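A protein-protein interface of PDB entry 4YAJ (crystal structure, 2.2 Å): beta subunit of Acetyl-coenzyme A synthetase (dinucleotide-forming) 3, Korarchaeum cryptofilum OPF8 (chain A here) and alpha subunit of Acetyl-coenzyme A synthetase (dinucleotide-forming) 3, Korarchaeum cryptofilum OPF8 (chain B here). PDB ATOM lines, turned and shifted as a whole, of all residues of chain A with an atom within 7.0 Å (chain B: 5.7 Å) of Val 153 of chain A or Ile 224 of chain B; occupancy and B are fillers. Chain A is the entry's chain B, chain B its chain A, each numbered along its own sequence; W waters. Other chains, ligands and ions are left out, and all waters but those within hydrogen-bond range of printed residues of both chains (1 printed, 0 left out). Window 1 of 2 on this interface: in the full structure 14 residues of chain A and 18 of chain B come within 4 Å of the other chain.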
ATOM      1  N   ASP A 127     -11.243 -19.401  14.741  1.00  0.00           N
ATOM      2  CA  ASP A 127     -10.154 -20.340  14.508  1.00  0.00           C
ATOM      3  C   ASP A 127      -8.864 -19.580  14.215  1.00  0.00           C
ATOM      4  O   ASP A 127      -8.895 -18.619  13.454  1.00  0.00           O
ATOM      5  CB  ASP A 127     -10.496 -21.267  13.343  1.00  0.00           C
ATOM      6  CG  ASP A 127      -9.458 -22.348  13.135  1.00  0.00           C
ATOM      7  OD1 ASP A 127      -9.455 -23.330  13.907  1.00  0.00           O
ATOM      8  OD2 ASP A 127      -8.642 -22.213  12.200  1.00  0.00           O
ATOM      9  N   PHE A 130      -8.332 -19.570  10.196  1.00  0.00           N
ATOM     10  CA  PHE A 130      -9.374 -19.144   9.269  1.00  0.00           C
ATOM     11  C   PHE A 130     -10.308 -18.074   9.832  1.00  0.00           C
ATOM     12  O   PHE A 130     -11.244 -17.654   9.158  1.00  0.00           O
ATOM     13  CB  PHE A 130     -10.184 -20.364   8.831  1.00  0.00           C
ATOM     14  CG  PHE A 130      -9.368 -21.392   8.105  1.00  0.00           C
ATOM     15  CD1 PHE A 130      -9.051 -21.228   6.769  1.00  0.00           C
ATOM     16  CD2 PHE A 130      -8.907 -22.519   8.764  1.00  0.00           C
ATOM     17  CE1 PHE A 130      -8.293 -22.169   6.102  1.00  0.00           C
ATOM     18  CE2 PHE A 130      -8.151 -23.465   8.102  1.00  0.00           C
ATOM     19  CZ  PHE A 130      -7.844 -23.290   6.769  1.00  0.00           C
ATOM     20  N   GLY A 131     -10.059 -17.637  11.062  1.00  0.00           N
ATOM     21  CA  GLY A 131     -10.872 -16.604  11.675  1.00  0.00           C
ATOM     22  C   GLY A 131     -12.302 -17.061  11.918  1.00  0.00           C
ATOM     23  O   GLY A 131     -12.543 -18.253  12.107  1.00  0.00           O
ATOM     24  N   PRO A 132     -13.268 -16.123  11.882  1.00  0.00           N
ATOM     25  CA  PRO A 132     -14.654 -16.453  12.243  1.00  0.00           C
ATOM     26  C   PRO A 132     -15.250 -17.613  11.440  1.00  0.00           C
ATOM     27  O   PRO A 132     -15.296 -17.577  10.209  1.00  0.00           O
ATOM     28  CB  PRO A 132     -15.416 -15.149  11.961  1.00  0.00           C
ATOM     29  CG  PRO A 132     -14.537 -14.352  11.082  1.00  0.00           C
ATOM     30  CD  PRO A 132     -13.141 -14.728  11.429  1.00  0.00           C
ATOM     31  N   THR A 133     -15.712 -18.627  12.165  1.00  0.00           N
ATOM     32  CA  THR A 133     -16.240 -19.850  11.574  1.00  0.00           C
ATOM     33  C   THR A 133     -17.594 -20.188  12.183  1.00  0.00           C
ATOM     34  O   THR A 133     -17.776 -20.087  13.394  1.00  0.00           O
ATOM     35  CB  THR A 133     -15.278 -21.033  11.790  1.00  0.00           C
ATOM     36  OG1 THR A 133     -13.984 -20.705  11.273  1.00  0.00           O
ATOM     37  CG2 THR A 133     -15.800 -22.295  11.113  1.00  0.00           C
ATOM     38  N   VAL A 134     -18.531 -20.607  11.341  1.00  0.00           N
ATOM     39  CA  VAL A 134     -19.876 -20.939  11.793  1.00  0.00           C
ATOM     40  C   VAL A 134     -20.019 -22.441  11.993  1.00  0.00           C
ATOM     41  O   VAL A 134     -19.536 -23.230  11.182  1.00  0.00           O
ATOM     42  CB  VAL A 134     -20.947 -20.458  10.789  1.00  0.00           C
ATOM     43  CG1 VAL A 134     -22.346 -20.819  11.274  1.00  0.00           C
ATOM     44  CG2 VAL A 134     -20.840 -18.960  10.572  1.00  0.00           C
ATOM     45  N   PHE A 151     -18.910 -27.319   9.818  1.00  0.00           N
ATOM     46  CA  PHE A 151     -18.266 -26.011   9.897  1.00  0.00           C
ATOM     47  C   PHE A 151     -18.166 -25.346   8.532  1.00  0.00           C
ATOM     48  O   PHE A 151     -17.965 -26.017   7.518  1.00  0.00           O
ATOM     49  CB  PHE A 151     -16.863 -26.132  10.493  1.00  0.00           C
ATOM     50  CG  PHE A 151     -16.839 -26.675  11.889  1.00  0.00           C
ATOM     51  CD1 PHE A 151     -16.961 -25.830  12.978  1.00  0.00           C
ATOM     52  CD2 PHE A 151     -16.676 -28.031  12.114  1.00  0.00           C
ATOM     53  CE1 PHE A 151     -16.932 -26.328  14.265  1.00  0.00           C
ATOM     54  CE2 PHE A 151     -16.645 -28.535  13.398  1.00  0.00           C
ATOM     55  CZ  PHE A 151     -16.774 -27.682  14.476  1.00  0.00           C
ATOM     56  N   ARG A 152     -18.304 -24.025   8.523  1.00  0.00           N
ATOM     57  CA  ARG A 152     -18.028 -23.217   7.340  1.00  0.00           C
ATOM     58  C   ARG A 152     -17.366 -21.904   7.748  1.00  0.00           C
ATOM     59  O   ARG A 152     -17.819 -21.233   8.673  1.00  0.00           O
ATOM     60  CB  ARG A 152     -19.312 -22.935   6.554  1.00  0.00           C
ATOM     61  CG  ARG A 152     -19.906 -24.137   5.834  1.00  0.00           C
ATOM     62  CD  ARG A 152     -19.015 -24.612   4.694  1.00  0.00           C
ATOM     63  NE  ARG A 152     -19.667 -25.634   3.881  1.00  0.00           N
ATOM     64  CZ  ARG A 152     -19.770 -26.915   4.218  1.00  0.00           C
ATOM     65  NH1 ARG A 152     -19.260 -27.353   5.363  1.00  0.00           N
ATOM     66  NH2 ARG A 152     -20.386 -27.764   3.409  1.00  0.00           N
ATOM     67  N   VAL A 153     -16.295 -21.543   7.051  1.00  0.00           N
ATOM     68  CA  VAL A 153     -15.587 -20.299   7.324  1.00  0.00           C
ATOM     69  C   VAL A 153     -16.382 -19.119   6.775  1.00  0.00           C
ATOM     70  O   VAL A 153     -16.839 -19.147   5.636  1.00  0.00           O
ATOM     71  CB  VAL A 153     -14.172 -20.308   6.710  1.00  0.00           C
ATOM     72  CG1 VAL A 153     -13.442 -19.005   7.008  1.00  0.00           C
ATOM     73  CG2 VAL A 153     -13.375 -21.491   7.232  1.00  0.00           C
ATOM     74  N   ALA A 154     -16.548 -18.085   7.594  1.00  0.00           N
ATOM     75  CA  ALA A 154     -17.354 -16.932   7.214  1.00  0.00           C
ATOM     76  C   ALA A 154     -16.542 -15.960   6.360  1.00  0.00           C
ATOM     77  O   ALA A 154     -15.320 -15.928   6.460  1.00  0.00           O
ATOM     78  CB  ALA A 154     -17.887 -16.233   8.454  1.00  0.00           C
ATOM     79  N   PRO A 155     -17.219 -15.157   5.519  1.00  0.00           N
ATOM     80  CA  PRO A 155     -18.674 -15.068   5.333  1.00  0.00           C
ATOM     81  C   PRO A 155     -19.273 -16.262   4.592  1.00  0.00           C
ATOM     82  O   PRO A 155     -18.620 -16.850   3.730  1.00  0.00           O
ATOM     83  CB  PRO A 155     -18.837 -13.790   4.507  1.00  0.00           C
ATOM     84  CG  PRO A 155     -17.569 -13.669   3.757  1.00  0.00           C
ATOM     85  CD  PRO A 155     -16.504 -14.185   4.675  1.00  0.00           C
ATOM     86  N   LEU A 156     -20.510 -16.604   4.935  1.00  0.00           N
ATOM     87  CA  LEU A 156     -21.195 -17.743   4.337  1.00  0.00           C
ATOM     88  C   LEU A 156     -22.016 -17.342   3.119  1.00  0.00           C
ATOM     89  O   LEU A 156     -22.764 -16.366   3.155  1.00  0.00           O
ATOM     90  CB  LEU A 156     -22.114 -18.411   5.361  1.00  0.00           C
ATOM     91  CG  LEU A 156     -21.516 -19.529   6.214  1.00  0.00           C
ATOM     92  CD1 LEU A 156     -20.329 -19.027   7.014  1.00  0.00           C
ATOM     93  CD2 LEU A 156     -22.577 -20.107   7.132  1.00  0.00           C
ATOM     94  N   SER A 157     -21.871 -18.107   2.044  1.00  0.00           N
ATOM     95  CA  SER A 157     -22.748 -17.989   0.890  1.00  0.00           C
ATOM     96  C   SER A 157     -23.987 -18.845   1.126  1.00  0.00           C
ATOM     97  O   SER A 157     -24.035 -19.630   2.074  1.00  0.00           O
ATOM     98  CB  SER A 157     -22.039 -18.439  -0.383  1.00  0.00           C
ATOM     99  OG  SER A 157     -21.853 -19.839  -0.341  1.00  0.00           O
ATOM    100  N   ASP A 160     -22.822 -22.292   0.884  1.00  0.00           N
ATOM    101  CA  ASP A 160     -22.151 -22.745   2.097  1.00  0.00           C
ATOM    102  C   ASP A 160     -23.169 -23.209   3.133  1.00  0.00           C
ATOM    103  O   ASP A 160     -23.029 -24.286   3.717  1.00  0.00           O
ATOM    104  CB  ASP A 160     -21.280 -21.631   2.684  1.00  0.00           C
ATOM    105  CG  ASP A 160     -20.019 -21.386   1.876  1.00  0.00           C
ATOM    106  OD1 ASP A 160     -19.384 -22.366   1.441  1.00  0.00           O
ATOM    107  OD2 ASP A 160     -19.669 -20.206   1.668  1.00  0.00           O
ATOM    108  N   MET A 164     -23.726 -27.178   4.291  1.00  0.00           N
ATOM    109  CA  MET A 164     -23.315 -27.521   5.648  1.00  0.00           C
ATOM    110  C   MET A 164     -24.501 -28.076   6.435  1.00  0.00           C
ATOM    111  O   MET A 164     -24.319 -28.888   7.339  1.00  0.00           O
ATOM    112  CB  MET A 164     -22.704 -26.313   6.371  1.00  0.00           C
ATOM    113  CG  MET A 164     -23.701 -25.340   6.981  1.00  0.00           C
ATOM    114  SD  MET A 164     -22.908 -23.900   7.720  1.00  0.00           S
ATOM    115  CE  MET A 164     -21.962 -24.661   9.035  1.00  0.00           C
ATOM    116  N   GLY A 196     -22.705 -15.742  10.558  1.00  0.00           N
ATOM    117  CA  GLY A 196     -21.393 -15.516   9.983  1.00  0.00           C
ATOM    118  C   GLY A 196     -21.076 -14.038   9.862  1.00  0.00           C
ATOM    119  O   GLY A 196     -19.960 -13.611  10.146  1.00  0.00           O
ATOM    120  N   VAL A 200     -17.960 -11.750  11.306  1.00  0.00           N
ATOM    121  CA  VAL A 200     -17.029 -11.015  10.457  1.00  0.00           C
ATOM    122  C   VAL A 200     -16.957  -9.546  10.868  1.00  0.00           C
ATOM    123  O   VAL A 200     -15.875  -8.970  10.944  1.00  0.00           O
ATOM    124  CB  VAL A 200     -17.428 -11.118   8.968  1.00  0.00           C
ATOM    125  CG1 VAL A 200     -16.592 -10.172   8.106  1.00  0.00           C
ATOM    126  CG2 VAL A 200     -17.269 -12.545   8.477  1.00  0.00           C
ATOM    127  N   ARG B 219      -3.934 -16.474   8.121  1.00  0.00           N
ATOM    128  CA  ARG B 219      -3.649 -16.574   6.691  1.00  0.00           C
ATOM    129  C   ARG B 219      -4.727 -17.378   5.963  1.00  0.00           C
ATOM    130  O   ARG B 219      -4.795 -17.375   4.733  1.00  0.00           O
ATOM    131  CB  ARG B 219      -2.275 -17.215   6.482  1.00  0.00           C
ATOM    132  CG  ARG B 219      -1.704 -17.089   5.078  1.00  0.00           C
ATOM    133  CD  ARG B 219      -1.425 -15.643   4.705  1.00  0.00           C
ATOM    134  NE  ARG B 219      -0.560 -15.548   3.532  1.00  0.00           N
ATOM    135  CZ  ARG B 219      -0.516 -14.506   2.706  1.00  0.00           C
ATOM    136  NH1 ARG B 219      -1.290 -13.449   2.911  1.00  0.00           N
ATOM    137  NH2 ARG B 219       0.309 -14.523   1.669  1.00  0.00           N
ATOM    138  N   GLY B 220      -5.578 -18.048   6.735  1.00  0.00           N
ATOM    139  CA  GLY B 220      -6.566 -18.963   6.190  1.00  0.00           C
ATOM    140  C   GLY B 220      -7.609 -18.335   5.282  1.00  0.00           C
ATOM    141  O   GLY B 220      -7.954 -18.901   4.244  1.00  0.00           O
ATOM    142  N   ARG B 221      -8.126 -17.175   5.674  1.00  0.00           N
ATOM    143  CA  ARG B 221      -9.169 -16.511   4.902  1.00  0.00           C
ATOM    144  C   ARG B 221      -8.661 -16.140   3.515  1.00  0.00           C
ATOM    145  O   ARG B 221      -9.330 -16.372   2.508  1.00  0.00           O
ATOM    146  CB  ARG B 221      -9.660 -15.261   5.636  1.00  0.00           C
ATOM    147  CG  ARG B 221     -10.783 -14.512   4.933  1.00  0.00           C
ATOM    148  CD  ARG B 221     -12.041 -15.356   4.820  1.00  0.00           C
ATOM    149  NE  ARG B 221     -12.281 -15.807   3.454  1.00  0.00           N
ATOM    150  CZ  ARG B 221     -13.337 -16.520   3.075  1.00  0.00           C
ATOM    151  NH1 ARG B 221     -14.261 -16.871   3.960  1.00  0.00           N
ATOM    152  NH2 ARG B 221     -13.471 -16.883   1.808  1.00  0.00           N
ATOM    153  N   MET B 222      -7.461 -15.576   3.472  1.00  0.00           N
ATOM    154  CA  MET B 222      -6.853 -15.175   2.216  1.00  0.00           C
ATOM    155  C   MET B 222      -6.533 -16.409   1.380  1.00  0.00           C
ATOM    156  O   MET B 222      -6.631 -16.382   0.153  1.00  0.00           O
ATOM    157  CB  MET B 222      -5.594 -14.354   2.481  1.00  0.00           C
ATOM    158  CG  MET B 222      -5.112 -13.542   1.293  1.00  0.00           C
ATOM    159  SD  MET B 222      -3.584 -12.638   1.621  1.00  0.00           S
ATOM    160  CE  MET B 222      -3.965 -11.815   3.170  1.00  0.00           C
ATOM    161  N   PHE B 223      -6.163 -17.495   2.055  1.00  0.00           N
ATOM    162  CA  PHE B 223      -5.897 -18.760   1.381  1.00  0.00           C
ATOM    163  C   PHE B 223      -7.138 -19.239   0.635  1.00  0.00           C
ATOM    164  O   PHE B 223      -7.048 -19.671  -0.510  1.00  0.00           O
ATOM    165  CB  PHE B 223      -5.434 -19.822   2.383  1.00  0.00           C
ATOM    166  CG  PHE B 223      -5.257 -21.189   1.785  1.00  0.00           C
ATOM    167  CD1 PHE B 223      -6.334 -22.051   1.660  1.00  0.00           C
ATOM    168  CD2 PHE B 223      -4.014 -21.614   1.353  1.00  0.00           C
ATOM    169  CE1 PHE B 223      -6.175 -23.306   1.113  1.00  0.00           C
ATOM    170  CE2 PHE B 223      -3.849 -22.869   0.805  1.00  0.00           C
ATOM    171  CZ  PHE B 223      -4.931 -23.716   0.685  1.00  0.00           C
ATOM    172  N   ILE B 224      -8.292 -19.174   1.292  1.00  0.00           N
ATOM    173  CA  ILE B 224      -9.541 -19.585   0.660  1.00  0.00           C
ATOM    174  C   ILE B 224      -9.884 -18.662  -0.503  1.00  0.00           C
ATOM    175  O   ILE B 224     -10.349 -19.112  -1.545  1.00  0.00           O
ATOM    176  CB  ILE B 224     -10.715 -19.600   1.659  1.00  0.00           C
ATOM    177  CG1 ILE B 224     -10.473 -20.649   2.744  1.00  0.00           C
ATOM    178  CG2 ILE B 224     -12.038 -19.881   0.935  1.00  0.00           C
ATOM    179  CD1 ILE B 224     -11.482 -20.620   3.875  1.00  0.00           C
ATOM    180  N   ASP B 225      -9.679 -17.362  -0.317  1.00  0.00           N
ATOM    181  CA  ASP B 225      -9.998 -16.396  -1.363  1.00  0.00           C
ATOM    182  C   ASP B 225      -9.166 -16.660  -2.616  1.00  0.00           C
ATOM    183  O   ASP B 225      -9.667 -16.604  -3.736  1.00  0.00           O
ATOM    184  CB  ASP B 225      -9.764 -14.967  -0.868  1.00  0.00           C
ATOM    185  CG  ASP B 225     -10.751 -14.550   0.209  1.00  0.00           C
ATOM    186  OD1 ASP B 225     -11.793 -15.219   0.363  1.00  0.00           O
ATOM    187  OD2 ASP B 225     -10.482 -13.547   0.902  1.00  0.00           O
ATOM    188  N   VAL B 226      -7.889 -16.966  -2.429  1.00  0.00           N
ATOM    189  CA  VAL B 226      -7.006 -17.178  -3.566  1.00  0.00           C
ATOM    190  C   VAL B 226      -7.249 -18.547  -4.196  1.00  0.00           C
ATOM    191  O   VAL B 226      -7.377 -18.656  -5.411  1.00  0.00           O
ATOM    192  CB  VAL B 226      -5.521 -17.041  -3.155  1.00  0.00           C
ATOM    193  CG1 VAL B 226      -4.584 -17.532  -4.258  1.00  0.00           C
ATOM    194  CG2 VAL B 226      -5.211 -15.597  -2.807  1.00  0.00           C
ATOM    195  N   ALA B 227      -7.330 -19.578  -3.364  1.00  0.00           N
ATOM    196  CA  ALA B 227      -7.473 -20.948  -3.843  1.00  0.00           C
ATOM    197  C   ALA B 227      -8.775 -21.177  -4.604  1.00  0.00           C
ATOM    198  O   ALA B 227      -8.816 -21.961  -5.548  1.00  0.00           O
ATOM    199  CB  ALA B 227      -7.377 -21.918  -2.677  1.00  0.00           C
ATOM    200  N   SER B 228      -9.849 -20.527  -4.170  1.00  0.00           N
ATOM    201  CA  SER B 228     -11.139 -20.675  -4.837  1.00  0.00           C
ATOM    202  C   SER B 228     -11.075 -20.112  -6.250  1.00  0.00           C
ATOM    203  O   SER B 228     -11.517 -20.747  -7.207  1.00  0.00           O
ATOM    204  CB  SER B 228     -12.246 -19.993  -4.035  1.00  0.00           C
ATOM    205  OG  SER B 228     -11.964 -18.624  -3.848  1.00  0.00           O
ATOM    206  N   ARG B 229     -10.518 -18.914  -6.380  1.00  0.00           N
ATOM    207  CA  ARG B 229     -10.436 -18.272  -7.680  1.00  0.00           C
ATOM    208  C   ARG B 229      -9.521 -19.065  -8.606  1.00  0.00           C
ATOM    209  O   ARG B 229      -9.841 -19.254  -9.779  1.00  0.00           O
ATOM    210  CB  ARG B 229      -9.953 -16.828  -7.534  1.00  0.00           C
ATOM    211  CG  ARG B 229     -11.106 -15.846  -7.402  1.00  0.00           C
ATOM    212  CD  ARG B 229     -10.865 -14.760  -6.371  1.00  0.00           C
ATOM    213  NE  ARG B 229     -12.138 -14.254  -5.865  1.00  0.00           N
ATOM    214  CZ  ARG B 229     -12.813 -14.791  -4.851  1.00  0.00           C
ATOM    215  NH1 ARG B 229     -13.967 -14.265  -4.477  1.00  0.00           N
ATOM    216  NH2 ARG B 229     -12.342 -15.848  -4.206  1.00  0.00           N
ATOM    217  N   ILE B 264     -12.128 -28.085  10.378  1.00  0.00           N
ATOM    218  CA  ILE B 264     -12.214 -26.754   9.802  1.00  0.00           C
ATOM    219  C   ILE B 264     -11.306 -26.656   8.580  1.00  0.00           C
ATOM    220  O   ILE B 264     -11.647 -25.988   7.609  1.00  0.00           O
ATOM    221  CB  ILE B 264     -11.862 -25.672  10.840  1.00  0.00           C
ATOM    222  CG1 ILE B 264     -12.870 -25.735  11.993  1.00  0.00           C
ATOM    223  CG2 ILE B 264     -11.858 -24.289  10.194  1.00  0.00           C
ATOM    224  CD1 ILE B 264     -12.632 -24.740  13.111  1.00  0.00           C
ATOM    225  N   SER B 267     -13.289 -28.166   5.805  1.00  0.00           N
ATOM    226  CA  SER B 267     -14.290 -27.218   5.336  1.00  0.00           C
ATOM    227  C   SER B 267     -13.663 -26.134   4.470  1.00  0.00           C
ATOM    228  O   SER B 267     -14.218 -25.755   3.442  1.00  0.00           O
ATOM    229  CB  SER B 267     -15.016 -26.586   6.522  1.00  0.00           C
ATOM    230  OG  SER B 267     -15.711 -27.567   7.267  1.00  0.00           O
ATOM    231  N   ALA B 268     -12.509 -25.637   4.903  1.00  0.00           N
ATOM    232  CA  ALA B 268     -11.787 -24.612   4.166  1.00  0.00           C
ATOM    233  C   ALA B 268     -11.405 -25.111   2.779  1.00  0.00           C
ATOM    234  O   ALA B 268     -11.450 -24.360   1.808  1.00  0.00           O
ATOM    235  CB  ALA B 268     -10.553 -24.184   4.930  1.00  0.00           C
ATOM    236  N   GLN B 271     -14.541 -25.180   0.581  1.00  0.00           N
ATOM    237  CA  GLN B 271     -14.917 -23.835   0.162  1.00  0.00           C
ATOM    238  C   GLN B 271     -13.938 -23.281  -0.867  1.00  0.00           C
ATOM    239  O   GLN B 271     -14.251 -22.330  -1.577  1.00  0.00           O
ATOM    240  CB  GLN B 271     -14.997 -22.905   1.372  1.00  0.00           C
ATOM    241  CG  GLN B 271     -16.092 -23.283   2.351  1.00  0.00           C
ATOM    242  CD  GLN B 271     -16.028 -22.487   3.640  1.00  0.00           C
ATOM    243  OE1 GLN B 271     -15.646 -23.009   4.683  1.00  0.00           O
ATOM    244  NE2 GLN B 271     -16.417 -21.220   3.574  1.00  0.00           N
ATOM    245  N   SER B 272     -12.758 -23.888  -0.943  1.00  0.00           N
ATOM    246  CA  SER B 272     -11.736 -23.486  -1.903  1.00  0.00           C
ATOM    247  C   SER B 272     -11.819 -24.288  -3.202  1.00  0.00           C
ATOM    248  O   SER B 272     -11.113 -23.993  -4.164  1.00  0.00           O
ATOM    249  CB  SER B 272     -10.345 -23.646  -1.292  1.00  0.00           C
ATOM    250  OG  SER B 272     -10.164 -22.765  -0.201  1.00  0.00           O
HETATM  251  O   HOH W   1     -18.099 -28.996   7.969  1.00  0.00           O
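The guanidinium group (NH1) of Arg 221 of chain B is in hydrogen-bond range of the backbone carbonyl oxygen (O) of Ala 154 of chain A, 2.9 Å away.
OG of Ser 267 of chain B lies within hydrogen-bond range of O of Phe 151 of chain A, at 2.7 Å.
OE1 of Gln 271 of chain B lies within hydrogen-bond range of N of Val 153 of chain A.
Of the printed residues of chain B, Arg 152 of chain A touches Gln 271 (3.6 Å).
Printed residues of chain A within 4 Å of Ile 264 of chain B: Asp 127 and Phe 130.
Printed residues of chain B within 4 Å of Ala 154 of chain A: Arg 221.
Printed residues of chain B within 4 Å of Asp 160 of chain A: Gln 271.
Asp 225 of chain B touches none of the printed residues of chain A.
Val 200 of chain A touches none of the printed residues of chain B.
The nearest residue of chain A that does not touch Ile 224 of chain B is Ala 154 of chain A (6.6 Å).
Printed residues of chain B that touch a printed residue of chain A: Gly 220, Arg 221, Ile 224, Ile 264, Ser 267, Ala 268 and Gln 271.
Hydrophobic or aromatic side chains of chain B that line the printed part of chain A: Ile 224, Ile 264 and Ala 268.
Of the 17 printed residues of chain A, 8 touch a printed residue of chain B.
Among the printed residues, no Asp or Glu carboxylate lies within 4 Å of a Lys or Arg side-chain nitrogen of the other chain.
Water W1 lies within hydrogen-bond range of the backbone NH (N) of Phe 151 of chain A (2.6 Å), the side-chain hydroxyl (OG) of Ser 267 of chain B (2.9 Å) and the guanidinium group (NH1) of Arg 152 of chain A (3.3 Å).
O of Ile 224 of chain B sits at hydrogen-bond distance from OG of Ser 228 of chain B, at 2.9 Å.
The backbone carbonyl oxygen of Ser 267 of chain B lies close to the side-chain amide oxygen of Gln 271 of chain B (3.3 Å).
The side-chain carboxylate (OD2) of Asp 127 of chain A is in hydrogen-bond range of the backbone NH (N) of Phe 130 of chain A, at 3.3 Å.
O of Pro 132 of chain A is in hydrogen-bond range of N of Ala 154 of chain A, at 2.9 Å.
O of Arg 152 of chain A lies within hydrogen-bond range of N of Val 134 of chain A, at 2.8 Å.
OG of Ser 157 of chain A lies within hydrogen-bond range of N of Asp 160 of chain A.
OD1 of Asp 127 of chain A touches CD1 of Ile 264 of chain B, at 3.6 Å.
CD1 of Phe 130 of chain A touches CA of Gly 220 of chain B (3.4 Å).
Phe 130 of chain A touches Ile 224 of chain B.
Ile 264 of chain B touches Phe 130 of chain A (CG2 to CD2, 3.7 Å).
CE1 of Phe 130 of chain A touches CB of Ala 268 of chain B, at 3.2 Å.
OE1 of Gln 271 of chain B touches CA of Arg 152 of chain A (3.6 Å).
Val 153 of chain A touches Arg 221 of chain B (CG1 to NH1, 3.8 Å).
Ile 224 of chain B touches Val 153 of chain A (CD1 to CB, 3.9 Å).
Arg 221 of chain B touches Pro 155 of chain A (NH1 to CD, 3.6 Å).
CG of Gln 271 of chain B touches OD1 of Asp 160 of chain A, 3.5 Å away.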
